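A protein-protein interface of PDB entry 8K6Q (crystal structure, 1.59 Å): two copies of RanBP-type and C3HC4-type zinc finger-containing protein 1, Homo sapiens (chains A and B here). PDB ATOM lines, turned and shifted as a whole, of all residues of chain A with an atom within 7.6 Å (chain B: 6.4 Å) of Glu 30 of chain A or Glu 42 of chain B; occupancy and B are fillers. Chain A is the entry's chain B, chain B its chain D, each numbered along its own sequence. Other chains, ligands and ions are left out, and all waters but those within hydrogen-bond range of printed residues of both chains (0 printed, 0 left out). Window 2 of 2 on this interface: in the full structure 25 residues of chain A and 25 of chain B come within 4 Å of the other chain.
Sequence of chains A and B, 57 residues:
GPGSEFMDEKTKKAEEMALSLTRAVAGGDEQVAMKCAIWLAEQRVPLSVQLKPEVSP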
ATOM      1  N   ALA A  24      23.164   7.142 -22.305  1.00  0.00           N
ATOM      2  CA  ALA A  24      24.211   6.193 -21.936  1.00  0.00           C
ATOM      3  C   ALA A  24      23.679   4.775 -21.896  1.00  0.00           C
ATOM      4  O   ALA A  24      24.318   3.845 -22.397  1.00  0.00           O
ATOM      5  CB  ALA A  24      24.821   6.569 -20.591  1.00  0.00           C
ATOM      6  N   VAL A  25      22.502   4.580 -21.299  1.00  0.00           N
ATOM      7  CA  VAL A  25      21.935   3.243 -21.251  1.00  0.00           C
ATOM      8  C   VAL A  25      21.641   2.731 -22.654  1.00  0.00           C
ATOM      9  O   VAL A  25      21.949   1.582 -22.986  1.00  0.00           O
ATOM     10  CB  VAL A  25      20.680   3.244 -20.367  1.00  0.00           C
ATOM     11  CG1 VAL A  25      19.921   1.930 -20.526  1.00  0.00           C
ATOM     12  CG2 VAL A  25      21.077   3.444 -18.935  1.00  0.00           C
ATOM     13  N   GLY A  27      23.064   3.409 -25.442  1.00  0.00           N
ATOM     14  CA  GLY A  27      24.293   3.126 -26.158  1.00  0.00           C
ATOM     15  C   GLY A  27      25.222   2.130 -25.503  1.00  0.00           C
ATOM     16  O   GLY A  27      26.323   1.885 -26.021  1.00  0.00           O
ATOM     17  N   GLY A  28      24.825   1.552 -24.373  1.00  0.00           N
ATOM     18  CA  GLY A  28      25.675   0.598 -23.686  1.00  0.00           C
ATOM     19  C   GLY A  28      26.879   1.198 -22.996  1.00  0.00           C
ATOM     20  O   GLY A  28      27.873   0.499 -22.783  1.00  0.00           O
ATOM     21  N   ASP A  29      26.816   2.479 -22.632  1.00  0.00           N
ATOM     22  CA  ASP A  29      27.925   3.171 -21.969  1.00  0.00           C
ATOM     23  C   ASP A  29      27.783   2.947 -20.467  1.00  0.00           C
ATOM     24  O   ASP A  29      27.219   3.769 -19.740  1.00  0.00           O
ATOM     25  CB  ASP A  29      27.920   4.651 -22.335  1.00  0.00           C
ATOM     26  CG  ASP A  29      29.230   5.337 -22.025  1.00  0.00           C
ATOM     27  OD1 ASP A  29      29.895   4.944 -21.040  1.00  0.00           O
ATOM     28  OD2 ASP A  29      29.590   6.273 -22.767  1.00  0.00           O
ATOM     29  N   GLU A  30      28.332   1.827 -19.993  1.00  0.00           N
ATOM     30  CA  GLU A  30      28.089   1.392 -18.621  1.00  0.00           C
ATOM     31  C   GLU A  30      28.696   2.350 -17.603  1.00  0.00           C
ATOM     32  O   GLU A  30      28.090   2.605 -16.552  1.00  0.00           O
ATOM     33  CB  GLU A  30      28.627  -0.030 -18.421  1.00  0.00           C
ATOM     34  CG  GLU A  30      28.024  -1.027 -19.405  1.00  0.00           C
ATOM     35  CD  GLU A  30      28.520  -2.443 -19.208  1.00  0.00           C
ATOM     36  OE1 GLU A  30      29.371  -2.657 -18.322  1.00  0.00           O
ATOM     37  OE2 GLU A  30      28.070  -3.337 -19.955  1.00  0.00           O
ATOM     38  N   GLN A  31      29.884   2.901 -17.892  1.00  0.00           N
ATOM     39  CA  GLN A  31      30.527   3.780 -16.920  1.00  0.00           C
ATOM     40  C   GLN A  31      29.750   5.076 -16.751  1.00  0.00           C
ATOM     41  O   GLN A  31      29.530   5.532 -15.622  1.00  0.00           O
ATOM     42  CB  GLN A  31      31.972   4.067 -17.334  1.00  0.00           C
ATOM     43  CG  GLN A  31      32.905   2.877 -17.149  1.00  0.00           C
ATOM     44  CD  GLN A  31      32.962   2.384 -15.709  1.00  0.00           C
ATOM     45  OE1 GLN A  31      33.211   3.156 -14.780  1.00  0.00           O
ATOM     46  NE2 GLN A  31      32.740   1.089 -15.521  1.00  0.00           N
ATOM     47  N   VAL A  32      29.314   5.678 -17.855  1.00  0.00           N
ATOM     48  CA  VAL A  32      28.553   6.917 -17.761  1.00  0.00           C
ATOM     49  C   VAL A  32      27.183   6.657 -17.137  1.00  0.00           C
ATOM     50  O   VAL A  32      26.688   7.461 -16.336  1.00  0.00           O
ATOM     51  CB  VAL A  32      28.434   7.573 -19.149  1.00  0.00           C
ATOM     52  CG1 VAL A  32      27.486   8.772 -19.103  1.00  0.00           C
ATOM     53  CG2 VAL A  32      29.811   7.990 -19.654  1.00  0.00           C
ATOM     54  N   ALA A  33      26.543   5.540 -17.493  1.00  0.00           N
ATOM     55  CA  ALA A  33      25.252   5.225 -16.882  1.00  0.00           C
ATOM     56  C   ALA A  33      25.366   5.131 -15.365  1.00  0.00           C
ATOM     57  O   ALA A  33      24.520   5.662 -14.635  1.00  0.00           O
ATOM     58  CB  ALA A  33      24.706   3.919 -17.464  1.00  0.00           C
ATOM     59  N   MET A  34      26.404   4.456 -14.864  1.00  0.00           N
ATOM     60  CA  MET A  34      26.562   4.345 -13.417  1.00  0.00           C
ATOM     61  C   MET A  34      26.810   5.704 -12.769  1.00  0.00           C
ATOM     62  O   MET A  34      26.253   5.997 -11.704  1.00  0.00           O
ATOM     63  CB  MET A  34      27.708   3.393 -13.072  1.00  0.00           C
ATOM     64  CG  MET A  34      27.349   1.935 -13.149  1.00  0.00           C
ATOM     65  SD  MET A  34      28.654   0.905 -12.433  1.00  0.00           S
ATOM     66  CE  MET A  34      29.997   1.235 -13.570  1.00  0.00           C
ATOM     67  N   LYS A  35      27.677   6.533 -13.369  1.00  0.00           N
ATOM     68  CA  LYS A  35      27.950   7.842 -12.773  1.00  0.00           C
ATOM     69  C   LYS A  35      26.708   8.725 -12.782  1.00  0.00           C
ATOM     70  O   LYS A  35      26.473   9.468 -11.821  1.00  0.00           O
ATOM     71  CB  LYS A  35      29.106   8.535 -13.489  1.00  0.00           C
ATOM     72  CG  LYS A  35      30.330   7.649 -13.602  1.00  0.00           C
ATOM     73  CD  LYS A  35      31.491   8.352 -14.284  1.00  0.00           C
ATOM     74  CE  LYS A  35      32.820   7.896 -13.703  1.00  0.00           C
ATOM     75  NZ  LYS A  35      32.938   6.408 -13.716  1.00  0.00           N
ATOM     76  N   CYS A  36      25.891   8.648 -13.842  1.00  0.00           N
ATOM     77  CA  CYS A  36      24.637   9.401 -13.861  1.00  0.00           C
ATOM     78  C   CYS A  36      23.688   8.917 -12.765  1.00  0.00           C
ATOM     79  O   CYS A  36      23.054   9.728 -12.076  1.00  0.00           O
ATOM     80  CB  CYS A  36      23.957   9.298 -15.230  1.00  0.00           C
ATOM     81  SG  CYS A  36      24.698  10.285 -16.525  1.00  0.00           S
ATOM     82  N   LYS B  10      13.998 -11.652 -19.826  1.00  0.00           N
ATOM     83  CA  LYS B  10      14.863 -10.486 -19.886  1.00  0.00           C
ATOM     84  C   LYS B  10      14.052  -9.202 -19.770  1.00  0.00           C
ATOM     85  O   LYS B  10      14.478  -8.255 -19.089  1.00  0.00           O
ATOM     86  CB  LYS B  10      15.660 -10.523 -21.186  1.00  0.00           C
ATOM     87  CG  LYS B  10      16.720  -9.466 -21.311  1.00  0.00           C
ATOM     88  CD  LYS B  10      18.079 -10.138 -21.364  1.00  0.00           C
ATOM     89  CE  LYS B  10      18.469 -10.642 -19.974  1.00  0.00           C
ATOM     90  NZ  LYS B  10      19.785 -11.335 -19.890  1.00  0.00           N
ATOM     91  N   ALA B  37      21.560   0.584 -13.051  1.00  0.00           N
ATOM     92  CA  ALA B  37      21.951   1.299 -14.255  1.00  0.00           C
ATOM     93  C   ALA B  37      22.914   0.482 -15.109  1.00  0.00           C
ATOM     94  O   ALA B  37      22.808   0.475 -16.341  1.00  0.00           O
ATOM     95  CB  ALA B  37      22.568   2.642 -13.870  1.00  0.00           C
ATOM     96  N   ILE B  38      23.853  -0.226 -14.479  1.00  0.00           N
ATOM     97  CA  ILE B  38      24.819  -0.952 -15.292  1.00  0.00           C
ATOM     98  C   ILE B  38      24.144  -2.128 -15.985  1.00  0.00           C
ATOM     99  O   ILE B  38      24.464  -2.443 -17.139  1.00  0.00           O
ATOM    100  CB  ILE B  38      26.049  -1.375 -14.461  1.00  0.00           C
ATOM    101  CG1 ILE B  38      27.210  -1.698 -15.398  1.00  0.00           C
ATOM    102  CG2 ILE B  38      25.750  -2.568 -13.572  1.00  0.00           C
ATOM    103  CD1 ILE B  38      28.468  -2.169 -14.696  1.00  0.00           C
ATOM    104  N   TRP B  39      23.174  -2.764 -15.328  1.00  0.00           N
ATOM    105  CA  TRP B  39      22.459  -3.855 -15.977  1.00  0.00           C
ATOM    106  C   TRP B  39      21.656  -3.343 -17.163  1.00  0.00           C
ATOM    107  O   TRP B  39      21.700  -3.923 -18.252  1.00  0.00           O
ATOM    108  CB  TRP B  39      21.531  -4.552 -14.985  1.00  0.00           C
ATOM    109  CG  TRP B  39      20.960  -5.846 -15.527  1.00  0.00           C
ATOM    110  CD1 TRP B  39      21.429  -7.108 -15.279  1.00  0.00           C
ATOM    111  CD2 TRP B  39      19.827  -6.009 -16.404  1.00  0.00           C
ATOM    112  NE1 TRP B  39      20.661  -8.037 -15.938  1.00  0.00           N
ATOM    113  CE2 TRP B  39      19.679  -7.391 -16.642  1.00  0.00           C
ATOM    114  CE3 TRP B  39      18.939  -5.124 -17.022  1.00  0.00           C
ATOM    115  CZ2 TRP B  39      18.668  -7.907 -17.457  1.00  0.00           C
ATOM    116  CZ3 TRP B  39      17.933  -5.634 -17.822  1.00  0.00           C
ATOM    117  CH2 TRP B  39      17.809  -7.017 -18.038  1.00  0.00           C
ATOM    118  N   LEU B  40      20.908  -2.255 -16.960  1.00  0.00           N
ATOM    119  CA  LEU B  40      20.129  -1.688 -18.054  1.00  0.00           C
ATOM    120  C   LEU B  40      21.030  -1.278 -19.214  1.00  0.00           C
ATOM    121  O   LEU B  40      20.686  -1.480 -20.389  1.00  0.00           O
ATOM    122  CB  LEU B  40      19.323  -0.489 -17.533  1.00  0.00           C
ATOM    123  CG  LEU B  40      18.200  -0.866 -16.554  1.00  0.00           C
ATOM    124  CD1 LEU B  40      17.702   0.363 -15.804  1.00  0.00           C
ATOM    125  CD2 LEU B  40      17.038  -1.567 -17.284  1.00  0.00           C
ATOM    126  N   ALA B  41      22.189  -0.695 -18.904  1.00  0.00           N
ATOM    127  CA  ALA B  41      23.107  -0.252 -19.946  1.00  0.00           C
ATOM    128  C   ALA B  41      23.689  -1.431 -20.713  1.00  0.00           C
ATOM    129  O   ALA B  41      23.801  -1.387 -21.941  1.00  0.00           O
ATOM    130  CB  ALA B  41      24.237   0.577 -19.334  1.00  0.00           C
ATOM    131  N   GLU B  42      24.056  -2.501 -20.008  1.00  0.00           N
ATOM    132  CA  GLU B  42      24.613  -3.661 -20.695  1.00  0.00           C
ATOM    133  C   GLU B  42      23.603  -4.252 -21.673  1.00  0.00           C
ATOM    134  O   GLU B  42      23.967  -4.674 -22.780  1.00  0.00           O
ATOM    135  CB  GLU B  42      25.069  -4.693 -19.665  1.00  0.00           C
ATOM    136  CG  GLU B  42      25.988  -5.751 -20.220  1.00  0.00           C
ATOM    137  CD  GLU B  42      25.273  -7.061 -20.407  1.00  0.00           C
ATOM    138  OE1 GLU B  42      24.586  -7.492 -19.456  1.00  0.00           O
ATOM    139  OE2 GLU B  42      25.393  -7.658 -21.498  1.00  0.00           O
ATOM    140  N   GLN B  43      22.317  -4.253 -21.300  1.00  0.00           N
ATOM    141  CA  GLN B  43      21.256  -4.730 -22.173  1.00  0.00           C
ATOM    142  C   GLN B  43      20.769  -3.673 -23.159  1.00  0.00           C
ATOM    143  O   GLN B  43      19.927  -3.988 -24.006  1.00  0.00           O
ATOM    144  CB  GLN B  43      20.082  -5.226 -21.326  1.00  0.00           C
ATOM    145  CG  GLN B  43      20.426  -6.446 -20.489  1.00  0.00           C
ATOM    146  CD  GLN B  43      20.789  -7.633 -21.341  1.00  0.00           C
ATOM    147  OE1 GLN B  43      20.056  -7.993 -22.262  1.00  0.00           O
ATOM    148  NE2 GLN B  43      21.931  -8.241 -21.053  1.00  0.00           N
ATOM    149  N   ARG B  44      21.272  -2.437 -23.061  1.00  0.00           N
ATOM    150  CA  ARG B  44      20.897  -1.336 -23.945  1.00  0.00           C
ATOM    151  C   ARG B  44      19.383  -1.157 -24.002  1.00  0.00           C
ATOM    152  O   ARG B  44      18.778  -1.043 -25.072  1.00  0.00           O
ATOM    153  CB  ARG B  44      21.492  -1.528 -25.336  1.00  0.00           C
ATOM    154  CG  ARG B  44      22.965  -1.874 -25.282  1.00  0.00           C
ATOM    155  CD  ARG B  44      23.655  -1.468 -26.548  1.00  0.00           C
ATOM    156  NE  ARG B  44      25.048  -1.896 -26.557  1.00  0.00           N
ATOM    157  CZ  ARG B  44      25.883  -1.644 -27.554  1.00  0.00           C
ATOM    158  NH1 ARG B  44      25.450  -0.976 -28.614  1.00  0.00           N
ATOM    159  NH2 ARG B  44      27.138  -2.064 -27.495  1.00  0.00           N
ATOM    160  N   VAL B  45      18.773  -1.128 -22.823  1.00  0.00           N
ATOM    161  CA  VAL B  45      17.326  -0.953 -22.697  1.00  0.00           C
ATOM    162  C   VAL B  45      16.933   0.479 -23.057  1.00  0.00           C
ATOM    163  O   VAL B  45      17.413   1.425 -22.417  1.00  0.00           O
ATOM    164  CB  VAL B  45      16.853  -1.292 -21.277  1.00  0.00           C
ATOM    165  CG1 VAL B  45      15.327  -1.204 -21.177  1.00  0.00           C
ATOM    166  CG2 VAL B  45      17.380  -2.660 -20.837  1.00  0.00           C
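The side-chain carboxylate (OE1) of Glu 42 of chain B is in hydrogen-bond range of the side-chain amide nitrogen (NE2) of Gln 43 of chain B (3.2 Å). O of Leu 40 of chain B lies within hydrogen-bond range of N of Val 45 of chain B (3.1 Å).
Leu 40 of chain B touches Val 25 of chain A (O to CG1, 3.5 Å). Ala 41 of chain B touches Val 25 of chain A. O of Val 25 of chain A touches CA of Arg 44 of chain B (3.2 Å). O of Val 45 of chain B touches CG1 of Val 25 of chain A, 3.2 Å away. O of Gly 27 of chain A touches CZ of Arg 44 of chain B, at 3.9 Å. Gly 28 of chain A touches Ala 41 of chain B. Glu 30 of chain A touches Glu 42 of chain B. CB of Ala 37 of chain B touches O of Ala 33 of chain A, at 3.7 Å. CB of Ala 33 of chain A touches CB of Ala 41 of chain B, 3.9 Å away. Ile 38 of chain B touches Met 34 of chain A.
Of the printed residues of chain B, Glu 30 of chain A touches Ile 38 (3.7 Å) and Glu 42 (3.2 Å). Glu 42 of chain B touches one residue of chain A. Of the printed residues of chain B, Met 34 of chain A touches Ile 38 (3.8 Å). Of the printed residues of chain B, Ala 33 of chain A touches Ala 37 and Ala 41. The nearest printed residue of chain B that does not touch Glu 30 of chain A is Ala 41 of chain B (4.001 Å). The nearest residue of chain A that does not touch Glu 42 of chain B is Gly 28 of chain A (5.1 Å). The nearest printed residue of chain B that does not touch Ala 33 of chain A is Ile 38 of chain B (5.2 Å).
Of the 12 printed residues of chain A, 6 touch a printed residue of chain B. Hydrophobic or aromatic side chains of chain A within 4 Å of the printed part of chain B: Val 25, Ala 33 and Met 34. Along chain A the printed residues that touch a printed residue of chain B span positions 25 to 34. Of the 10 printed residues of chain B, 7 touch a printed residue of chain A. Printed residues of chain B that touch a printed residue of chain A: Ala 37, Ile 38, Leu 40, Ala 41, Glu 42, Arg 44 and Val 45. Among the printed residues, 12 pairs touch across the chains.
No position is printed for both chains. Of the 12 pairs that touch across the chains among the printed residues, none has its exchanged pair printed and touching as well.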
